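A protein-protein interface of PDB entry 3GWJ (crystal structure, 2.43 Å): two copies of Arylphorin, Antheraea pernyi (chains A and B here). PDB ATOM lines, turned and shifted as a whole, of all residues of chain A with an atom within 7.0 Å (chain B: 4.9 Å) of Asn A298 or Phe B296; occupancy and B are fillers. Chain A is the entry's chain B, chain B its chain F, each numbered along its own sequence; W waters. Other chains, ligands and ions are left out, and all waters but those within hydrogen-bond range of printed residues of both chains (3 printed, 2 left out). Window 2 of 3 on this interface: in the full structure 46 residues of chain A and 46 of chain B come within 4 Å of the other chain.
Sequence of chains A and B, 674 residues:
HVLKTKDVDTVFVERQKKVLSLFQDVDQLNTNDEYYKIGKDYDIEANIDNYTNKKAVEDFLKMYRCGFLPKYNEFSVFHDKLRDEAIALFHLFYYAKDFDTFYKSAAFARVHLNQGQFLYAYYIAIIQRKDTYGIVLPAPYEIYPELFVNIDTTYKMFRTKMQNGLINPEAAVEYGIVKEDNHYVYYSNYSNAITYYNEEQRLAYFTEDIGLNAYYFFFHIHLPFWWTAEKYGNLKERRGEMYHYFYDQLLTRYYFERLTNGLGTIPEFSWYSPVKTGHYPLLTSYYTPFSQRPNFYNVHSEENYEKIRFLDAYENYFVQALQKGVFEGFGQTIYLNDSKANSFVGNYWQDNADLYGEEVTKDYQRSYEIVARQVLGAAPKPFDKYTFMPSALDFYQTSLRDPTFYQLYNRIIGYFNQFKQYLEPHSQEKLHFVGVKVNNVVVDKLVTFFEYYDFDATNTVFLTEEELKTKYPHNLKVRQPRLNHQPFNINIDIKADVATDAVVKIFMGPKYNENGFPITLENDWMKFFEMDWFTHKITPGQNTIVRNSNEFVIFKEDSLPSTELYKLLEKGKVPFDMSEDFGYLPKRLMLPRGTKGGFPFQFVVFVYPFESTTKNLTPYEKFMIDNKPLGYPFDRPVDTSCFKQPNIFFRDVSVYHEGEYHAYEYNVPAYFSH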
ATOM      1  N   TYR A 272      29.324  17.364  14.154  1.00  0.00           N
ATOM      2  CA  TYR A 272      29.291  17.165  12.711  1.00  0.00           C
ATOM      3  C   TYR A 272      28.876  15.782  12.236  1.00  0.00           C
ATOM      4  O   TYR A 272      28.914  15.493  11.046  1.00  0.00           O
ATOM      5  CB  TYR A 272      30.652  17.534  12.116  1.00  0.00           C
ATOM      6  CG  TYR A 272      31.036  18.976  12.381  1.00  0.00           C
ATOM      7  CD1 TYR A 272      31.689  19.352  13.560  1.00  0.00           C
ATOM      8  CD2 TYR A 272      30.714  19.973  11.463  1.00  0.00           C
ATOM      9  CE1 TYR A 272      32.010  20.689  13.811  1.00  0.00           C
ATOM     10  CE2 TYR A 272      31.026  21.311  11.705  1.00  0.00           C
ATOM     11  CZ  TYR A 272      31.670  21.662  12.872  1.00  0.00           C
ATOM     12  OH  TYR A 272      31.956  22.992  13.077  1.00  0.00           O
ATOM     13  N   SER A 273      28.465  14.937  13.171  1.00  0.00           N
ATOM     14  CA  SER A 273      28.044  13.584  12.850  1.00  0.00           C
ATOM     15  C   SER A 273      26.766  13.293  13.591  1.00  0.00           C
ATOM     16  O   SER A 273      26.494  13.887  14.635  1.00  0.00           O
ATOM     17  CB  SER A 273      29.111  12.577  13.265  1.00  0.00           C
ATOM     18  OG  SER A 273      30.306  12.832  12.552  1.00  0.00           O
ATOM     19  N   PRO A 274      25.958  12.375  13.059  1.00  0.00           N
ATOM     20  CA  PRO A 274      24.699  12.037  13.714  1.00  0.00           C
ATOM     21  C   PRO A 274      24.918  11.672  15.174  1.00  0.00           C
ATOM     22  O   PRO A 274      25.854  10.943  15.490  1.00  0.00           O
ATOM     23  CB  PRO A 274      24.200  10.852  12.892  1.00  0.00           C
ATOM     24  CG  PRO A 274      24.741  11.144  11.522  1.00  0.00           C
ATOM     25  CD  PRO A 274      26.156  11.569  11.844  1.00  0.00           C
ATOM     26  N   VAL A 275      24.073  12.199  16.058  1.00  0.00           N
ATOM     27  CA  VAL A 275      24.165  11.873  17.480  1.00  0.00           C
ATOM     28  C   VAL A 275      23.513  10.508  17.601  1.00  0.00           C
ATOM     29  O   VAL A 275      22.349  10.336  17.250  1.00  0.00           O
ATOM     30  CB  VAL A 275      23.405  12.870  18.359  1.00  0.00           C
ATOM     31  CG1 VAL A 275      23.538  12.473  19.794  1.00  0.00           C
ATOM     32  CG2 VAL A 275      23.951  14.265  18.157  1.00  0.00           C
ATOM     33  N   ARG A 293      14.172  13.253  19.981  1.00  0.00           N
ATOM     34  CA  ARG A 293      15.403  13.156  19.202  1.00  0.00           C
ATOM     35  C   ARG A 293      15.545  11.678  18.892  1.00  0.00           C
ATOM     36  O   ARG A 293      15.759  10.857  19.787  1.00  0.00           O
ATOM     37  CB  ARG A 293      16.623  13.611  20.000  1.00  0.00           C
ATOM     38  CG  ARG A 293      17.909  13.679  19.168  1.00  0.00           C
ATOM     39  CD  ARG A 293      19.102  13.310  20.026  1.00  0.00           C
ATOM     40  NE  ARG A 293      18.984  13.997  21.293  1.00  0.00           N
ATOM     41  CZ  ARG A 293      18.947  13.407  22.476  1.00  0.00           C
ATOM     42  NH1 ARG A 293      19.029  12.094  22.597  1.00  0.00           N
ATOM     43  NH2 ARG A 293      18.785  14.154  23.545  1.00  0.00           N
ATOM     44  N   PRO A 294      15.419  11.311  17.616  1.00  0.00           N
ATOM     45  CA  PRO A 294      15.543   9.894  17.285  1.00  0.00           C
ATOM     46  C   PRO A 294      16.990   9.451  17.303  1.00  0.00           C
ATOM     47  O   PRO A 294      17.898  10.287  17.253  1.00  0.00           O
ATOM     48  CB  PRO A 294      14.942   9.819  15.892  1.00  0.00           C
ATOM     49  CG  PRO A 294      15.394  11.132  15.294  1.00  0.00           C
ATOM     50  CD  PRO A 294      15.112  12.116  16.421  1.00  0.00           C
ATOM     51  N   ASN A 295      17.201   8.138  17.376  1.00  0.00           N
ATOM     52  CA  ASN A 295      18.552   7.596  17.358  1.00  0.00           C
ATOM     53  C   ASN A 295      19.227   8.054  16.064  1.00  0.00           C
ATOM     54  O   ASN A 295      18.577   8.205  15.034  1.00  0.00           O
ATOM     55  CB  ASN A 295      18.505   6.067  17.401  1.00  0.00           C
ATOM     56  CG  ASN A 295      17.951   5.535  18.711  1.00  0.00           C
ATOM     57  OD1 ASN A 295      17.306   4.490  18.739  1.00  0.00           O
ATOM     58  ND2 ASN A 295      18.214   6.247  19.809  1.00  0.00           N
ATOM     59  N   PHE A 296      20.532   8.282  16.131  1.00  0.00           N
ATOM     60  CA  PHE A 296      21.305   8.698  14.969  1.00  0.00           C
ATOM     61  C   PHE A 296      20.736   9.977  14.343  1.00  0.00           C
ATOM     62  O   PHE A 296      20.573  10.079  13.135  1.00  0.00           O
ATOM     63  CB  PHE A 296      21.335   7.535  13.965  1.00  0.00           C
ATOM     64  CG  PHE A 296      21.890   6.257  14.547  1.00  0.00           C
ATOM     65  CD1 PHE A 296      23.262   6.119  14.781  1.00  0.00           C
ATOM     66  CD2 PHE A 296      21.039   5.227  14.939  1.00  0.00           C
ATOM     67  CE1 PHE A 296      23.779   4.979  15.402  1.00  0.00           C
ATOM     68  CE2 PHE A 296      21.538   4.079  15.562  1.00  0.00           C
ATOM     69  CZ  PHE A 296      22.914   3.954  15.796  1.00  0.00           C
ATOM     70  N   TYR A 297      20.445  10.949  15.198  1.00  0.00           N
ATOM     71  CA  TYR A 297      19.886  12.228  14.790  1.00  0.00           C
ATOM     72  C   TYR A 297      20.863  13.086  13.984  1.00  0.00           C
ATOM     73  O   TYR A 297      21.965  13.390  14.434  1.00  0.00           O
ATOM     74  CB  TYR A 297      19.425  12.982  16.036  1.00  0.00           C
ATOM     75  CG  TYR A 297      18.950  14.398  15.799  1.00  0.00           C
ATOM     76  CD1 TYR A 297      17.834  14.664  15.010  1.00  0.00           C
ATOM     77  CD2 TYR A 297      19.603  15.473  16.407  1.00  0.00           C
ATOM     78  CE1 TYR A 297      17.379  15.978  14.838  1.00  0.00           C
ATOM     79  CE2 TYR A 297      19.163  16.765  16.247  1.00  0.00           C
ATOM     80  CZ  TYR A 297      18.052  17.023  15.466  1.00  0.00           C
ATOM     81  OH  TYR A 297      17.620  18.327  15.343  1.00  0.00           O
ATOM     82  N   ASN A 298      20.445  13.463  12.783  1.00  0.00           N
ATOM     83  CA  ASN A 298      21.261  14.297  11.904  1.00  0.00           C
ATOM     84  C   ASN A 298      21.256  15.721  12.476  1.00  0.00           C
ATOM     85  O   ASN A 298      20.424  16.555  12.112  1.00  0.00           O
ATOM     86  CB  ASN A 298      20.676  14.247  10.489  1.00  0.00           C
ATOM     87  CG  ASN A 298      21.278  15.281   9.571  1.00  0.00           C
ATOM     88  OD1 ASN A 298      22.443  15.659   9.727  1.00  0.00           O
ATOM     89  ND2 ASN A 298      20.492  15.739   8.594  1.00  0.00           N
ATOM     90  N   VAL A 299      22.183  15.977  13.393  1.00  0.00           N
ATOM     91  CA  VAL A 299      22.282  17.265  14.070  1.00  0.00           C
ATOM     92  C   VAL A 299      22.849  18.389  13.203  1.00  0.00           C
ATOM     93  O   VAL A 299      22.446  19.548  13.323  1.00  0.00           O
ATOM     94  CB  VAL A 299      23.122  17.115  15.376  1.00  0.00           C
ATOM     95  CG1 VAL A 299      24.552  16.739  15.045  1.00  0.00           C
ATOM     96  CG2 VAL A 299      23.068  18.385  16.184  1.00  0.00           C
ATOM     97  N   HIS A 300      23.768  18.041  12.313  1.00  0.00           N
ATOM     98  CA  HIS A 300      24.401  19.017  11.432  1.00  0.00           C
ATOM     99  C   HIS A 300      23.493  19.395  10.258  1.00  0.00           C
ATOM    100  O   HIS A 300      23.724  18.983   9.123  1.00  0.00           O
ATOM    101  CB  HIS A 300      25.727  18.436  10.912  1.00  0.00           C
ATOM    102  CG  HIS A 300      26.575  19.412  10.152  1.00  0.00           C
ATOM    103  ND1 HIS A 300      27.183  20.498  10.746  1.00  0.00           N
ATOM    104  CD2 HIS A 300      26.921  19.458   8.843  1.00  0.00           C
ATOM    105  CE1 HIS A 300      27.862  21.172   9.838  1.00  0.00           C
ATOM    106  NE2 HIS A 300      27.720  20.563   8.675  1.00  0.00           N
ATOM    107  N   SER A 301      22.452  20.173  10.523  1.00  0.00           N
ATOM    108  CA  SER A 301      21.547  20.591   9.450  1.00  0.00           C
ATOM    109  C   SER A 301      21.546  22.109   9.336  1.00  0.00           C
ATOM    110  O   SER A 301      22.128  22.800  10.172  1.00  0.00           O
ATOM    111  CB  SER A 301      20.123  20.102   9.708  1.00  0.00           C
ATOM    112  OG  SER A 301      19.556  20.799  10.800  1.00  0.00           O
ATOM    113  N   GLU A 302      20.890  22.629   8.305  1.00  0.00           N
ATOM    114  CA  GLU A 302      20.849  24.066   8.105  1.00  0.00           C
ATOM    115  C   GLU A 302      20.459  24.841   9.367  1.00  0.00           C
ATOM    116  O   GLU A 302      21.121  25.821   9.726  1.00  0.00           O
ATOM    117  CB  GLU A 302      19.898  24.421   6.964  1.00  0.00           C
ATOM    118  CG  GLU A 302      19.708  25.923   6.811  1.00  0.00           C
ATOM    119  CD  GLU A 302      18.981  26.309   5.540  1.00  0.00           C
ATOM    120  OE1 GLU A 302      18.779  27.534   5.321  1.00  0.00           O
ATOM    121  OE2 GLU A 302      18.620  25.387   4.767  1.00  0.00           O
ATOM    122  N   GLU A 303      19.395  24.409  10.039  1.00  0.00           N
ATOM    123  CA  GLU A 303      18.942  25.086  11.253  1.00  0.00           C
ATOM    124  C   GLU A 303      20.021  25.238  12.327  1.00  0.00           C
ATOM    125  O   GLU A 303      19.949  26.151  13.143  1.00  0.00           O
ATOM    126  CB  GLU A 303      17.738  24.357  11.857  1.00  0.00           C
ATOM    127  CG  GLU A 303      18.000  22.881  12.147  1.00  0.00           C
ATOM    128  CD  GLU A 303      16.771  22.133  12.671  1.00  0.00           C
ATOM    129  OE1 GLU A 303      16.473  22.233  13.889  1.00  0.00           O
ATOM    130  OE2 GLU A 303      16.106  21.447  11.850  1.00  0.00           O
ATOM    131  N   ASN A 304      21.021  24.357  12.327  1.00  0.00           N
ATOM    132  CA  ASN A 304      22.076  24.424  13.334  1.00  0.00           C
ATOM    133  C   ASN A 304      23.480  24.838  12.873  1.00  0.00           C
ATOM    134  O   ASN A 304      24.371  24.977  13.710  1.00  0.00           O
ATOM    135  CB  ASN A 304      22.193  23.086  14.076  1.00  0.00           C
ATOM    136  CG  ASN A 304      20.912  22.693  14.806  1.00  0.00           C
ATOM    137  OD1 ASN A 304      20.180  23.537  15.312  1.00  0.00           O
ATOM    138  ND2 ASN A 304      20.656  21.403  14.877  1.00  0.00           N
ATOM    139  N   PRO B 274      18.585  11.641   3.630  1.00  0.00           N
ATOM    140  CA  PRO B 274      17.676  12.153   4.663  1.00  0.00           C
ATOM    141  C   PRO B 274      16.348  12.621   4.053  1.00  0.00           C
ATOM    142  O   PRO B 274      16.324  13.167   2.946  1.00  0.00           O
ATOM    143  CB  PRO B 274      18.463  13.309   5.275  1.00  0.00           C
ATOM    144  CG  PRO B 274      19.908  12.904   5.057  1.00  0.00           C
ATOM    145  CD  PRO B 274      19.881  12.344   3.655  1.00  0.00           C
ATOM    146  N   VAL B 275      15.249  12.387   4.761  1.00  0.00           N
ATOM    147  CA  VAL B 275      13.938  12.816   4.282  1.00  0.00           C
ATOM    148  C   VAL B 275      13.802  14.272   4.712  1.00  0.00           C
ATOM    149  O   VAL B 275      13.819  14.587   5.894  1.00  0.00           O
ATOM    150  CB  VAL B 275      12.820  11.979   4.915  1.00  0.00           C
ATOM    151  CG1 VAL B 275      11.466  12.495   4.464  1.00  0.00           C
ATOM    152  CG2 VAL B 275      13.003  10.516   4.538  1.00  0.00           C
ATOM    153  N   LYS B 276      13.659  15.165   3.748  1.00  0.00           N
ATOM    154  CA  LYS B 276      13.597  16.579   4.060  1.00  0.00           C
ATOM    155  C   LYS B 276      12.466  17.098   4.939  1.00  0.00           C
ATOM    156  O   LYS B 276      12.714  17.771   5.946  1.00  0.00           O
ATOM    157  CB  LYS B 276      13.620  17.393   2.768  1.00  0.00           C
ATOM    158  CG  LYS B 276      13.613  18.896   3.008  1.00  0.00           C
ATOM    159  CD  LYS B 276      13.458  19.681   1.710  1.00  0.00           C
ATOM    160  CE  LYS B 276      13.395  21.173   1.980  1.00  0.00           C
ATOM    161  NZ  LYS B 276      13.096  21.935   0.734  1.00  0.00           N
ATOM    162  N   THR B 277      11.233  16.797   4.559  1.00  0.00           N
ATOM    163  CA  THR B 277      10.085  17.319   5.283  1.00  0.00           C
ATOM    164  C   THR B 277       9.659  16.549   6.521  1.00  0.00           C
ATOM    165  O   THR B 277       9.050  15.484   6.437  1.00  0.00           O
ATOM    166  CB  THR B 277       8.882  17.482   4.322  1.00  0.00           C
ATOM    167  OG1 THR B 277       8.462  16.194   3.856  1.00  0.00           O
ATOM    168  CG2 THR B 277       9.286  18.326   3.115  1.00  0.00           C
ATOM    169  N   PRO B 294      11.853  14.696  12.688  1.00  0.00           N
ATOM    170  CA  PRO B 294      12.442  16.015  12.446  1.00  0.00           C
ATOM    171  C   PRO B 294      12.782  16.225  10.980  1.00  0.00           C
ATOM    172  O   PRO B 294      12.841  15.275  10.210  1.00  0.00           O
ATOM    173  CB  PRO B 294      13.690  15.994  13.315  1.00  0.00           C
ATOM    174  CG  PRO B 294      14.105  14.555  13.245  1.00  0.00           C
ATOM    175  CD  PRO B 294      12.774  13.844  13.457  1.00  0.00           C
ATOM    176  N   ASN B 295      12.980  17.476  10.593  1.00  0.00           N
ATOM    177  CA  ASN B 295      13.344  17.790   9.223  1.00  0.00           C
ATOM    178  C   ASN B 295      14.694  17.101   8.924  1.00  0.00           C
ATOM    179  O   ASN B 295      15.525  16.934   9.825  1.00  0.00           O
ATOM    180  CB  ASN B 295      13.480  19.313   9.060  1.00  0.00           C
ATOM    181  CG  ASN B 295      12.170  20.059   9.338  1.00  0.00           C
ATOM    182  OD1 ASN B 295      12.172  21.113   9.984  1.00  0.00           O
ATOM    183  ND2 ASN B 295      11.053  19.522   8.844  1.00  0.00           N
ATOM    184  N   PHE B 296      14.902  16.701   7.671  1.00  0.00           N
ATOM    185  CA  PHE B 296      16.139  16.043   7.265  1.00  0.00           C
ATOM    186  C   PHE B 296      16.424  14.836   8.138  1.00  0.00           C
ATOM    187  O   PHE B 296      17.543  14.638   8.611  1.00  0.00           O
ATOM    188  CB  PHE B 296      17.297  17.033   7.337  1.00  0.00           C
ATOM    189  CG  PHE B 296      17.053  18.278   6.551  1.00  0.00           C
ATOM    190  CD1 PHE B 296      17.242  18.290   5.174  1.00  0.00           C
ATOM    191  CD2 PHE B 296      16.546  19.420   7.177  1.00  0.00           C
ATOM    192  CE1 PHE B 296      16.925  19.422   4.421  1.00  0.00           C
ATOM    193  CE2 PHE B 296      16.227  20.557   6.441  1.00  0.00           C
ATOM    194  CZ  PHE B 296      16.412  20.563   5.057  1.00  0.00           C
ATOM    195  N   TYR B 297      15.393  14.025   8.332  1.00  0.00           N
ATOM    196  CA  TYR B 297      15.487  12.824   9.140  1.00  0.00           C
ATOM    197  C   TYR B 297      16.383  11.798   8.464  1.00  0.00           C
ATOM    198  O   TYR B 297      16.233  11.525   7.266  1.00  0.00           O
ATOM    199  CB  TYR B 297      14.082  12.254   9.348  1.00  0.00           C
ATOM    200  CG  TYR B 297      14.015  10.879   9.962  1.00  0.00           C
ATOM    201  CD1 TYR B 297      14.497  10.647  11.242  1.00  0.00           C
ATOM    202  CD2 TYR B 297      13.404   9.820   9.283  1.00  0.00           C
ATOM    203  CE1 TYR B 297      14.369   9.406  11.843  1.00  0.00           C
ATOM    204  CE2 TYR B 297      13.267   8.569   9.876  1.00  0.00           C
ATOM    205  CZ  TYR B 297      13.750   8.370  11.161  1.00  0.00           C
ATOM    206  OH  TYR B 297      13.577   7.157  11.790  1.00  0.00           O
ATOM    207  N   ASN B 298      17.322  11.250   9.241  1.00  0.00           N
ATOM    208  CA  ASN B 298      18.256  10.224   8.769  1.00  0.00           C
ATOM    209  C   ASN B 298      17.516   8.875   8.753  1.00  0.00           C
ATOM    210  O   ASN B 298      17.605   8.093   9.698  1.00  0.00           O
ATOM    211  CB  ASN B 298      19.472  10.173   9.708  1.00  0.00           C
ATOM    212  CG  ASN B 298      20.432   9.037   9.377  1.00  0.00           C
ATOM    213  OD1 ASN B 298      20.573   8.634   8.212  1.00  0.00           O
ATOM    214  ND2 ASN B 298      21.112   8.524  10.403  1.00  0.00           N
HETATM  215  O   HOH W   1      17.510  12.450  11.882  1.00  0.00           O
HETATM  216  O   HOH W   2      13.516  22.316  12.712  1.00  0.00           O
HETATM  217  O   HOH W   3      16.118  18.639  12.101  1.00  0.00           O
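The backbone carbonyl oxygen (O) of Phe A296 lies within hydrogen-bond range of the side-chain amide nitrogen (ND2) of Asn B298 (3.2 Å).
The side-chain amide nitrogen of Asn A298 is in hydrogen-bond range of the backbone carbonyl oxygen of Phe B296 (3.1 Å).
The backbone NH of Phe A296 lies within hydrogen-bond range of the backbone carbonyl oxygen of Val A275, at 3.0 Å.
O of Val A275 sits at hydrogen-bond distance from N of Tyr A297 (2.9 Å).
N of Phe B296 lies within hydrogen-bond range of O of Val B275, at 3.0 Å.
The backbone NH (N) of Val B275 is in hydrogen-bond range of the backbone carbonyl oxygen (O) of Tyr B297 (2.8 Å).
The backbone NH (N) of Phe B296 lies within hydrogen-bond range of the backbone carbonyl oxygen (O) of Lys B276 (3.0 Å).
Among the printed residues, merely in contact across the chains: Pro A294 with Tyr B297 and Tyr A297 with Pro B294.
Asn A298 touches one residue of chain B.
Of chain A, only Asn A298 comes within 4 Å of Phe B296.
Of the printed residues of chain A, Pro B294 touches Tyr A297.
Of the printed residues of chain B, Phe A296 touches Asn B298.
Of the printed residues of chain B, Tyr A297 touches Pro B294 (3.9 Å).
The nearest residue of chain B that does not touch Asn A298 is Asn B298 (4.3 Å).
The nearest residue of chain A that does not touch Phe B296 is Ser A301 (4.4 Å).
The nearest printed residue of chain A that does not touch Asn B298 is Asn A298 (4.3 Å).
Of the 16 printed residues of chain A, 4 touch a printed residue of chain B.
Printed residues of chain A that touch a printed residue of chain B: Pro A294, Phe A296, Tyr A297 and Asn A298.
Hydrophobic or aromatic side chains of chain A that line the printed part of chain B: Pro A294, Phe A296 and Tyr A297.
Of the 9 printed residues of chain B, 4 touch a printed residue of chain A.
Hydrophobic or aromatic side chains of chain B that line the printed part of chain A: Pro B294, Phe B296 and Tyr B297.
Among the printed residues, no Asp or Glu carboxylate lies within 4 Å of a Lys or Arg side-chain nitrogen of the other chain.
Pro A294 touches Tyr B297, and with the chains exchanged Tyr A297 touches Pro B294.
Phe A296 touches Asn B298, and with the chains exchanged Asn A298 touches Phe B296.
Positions printed for both chains: 274, 275, 294, 295, 296, 297 and 298.
Of the 4 pairs that touch across the chains among the printed residues, 4 have their exchanged pair printed and touching as well.
Water W3 lies within hydrogen-bond range of the side-chain carboxylate (OE2) of Glu A303 (2.8 Å) and the backbone carbonyl oxygen (O) of Asn B295 (2.9 Å).
Water W2 lies within hydrogen-bond range of the side-chain carboxylate (OE2) of Glu A303 (2.9 Å) and the side-chain amide oxygen (OD1) of Asn B295 (3.3 Å).
Water W1 lies within hydrogen-bond range of N of Asn B298 and N of Asn A298.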
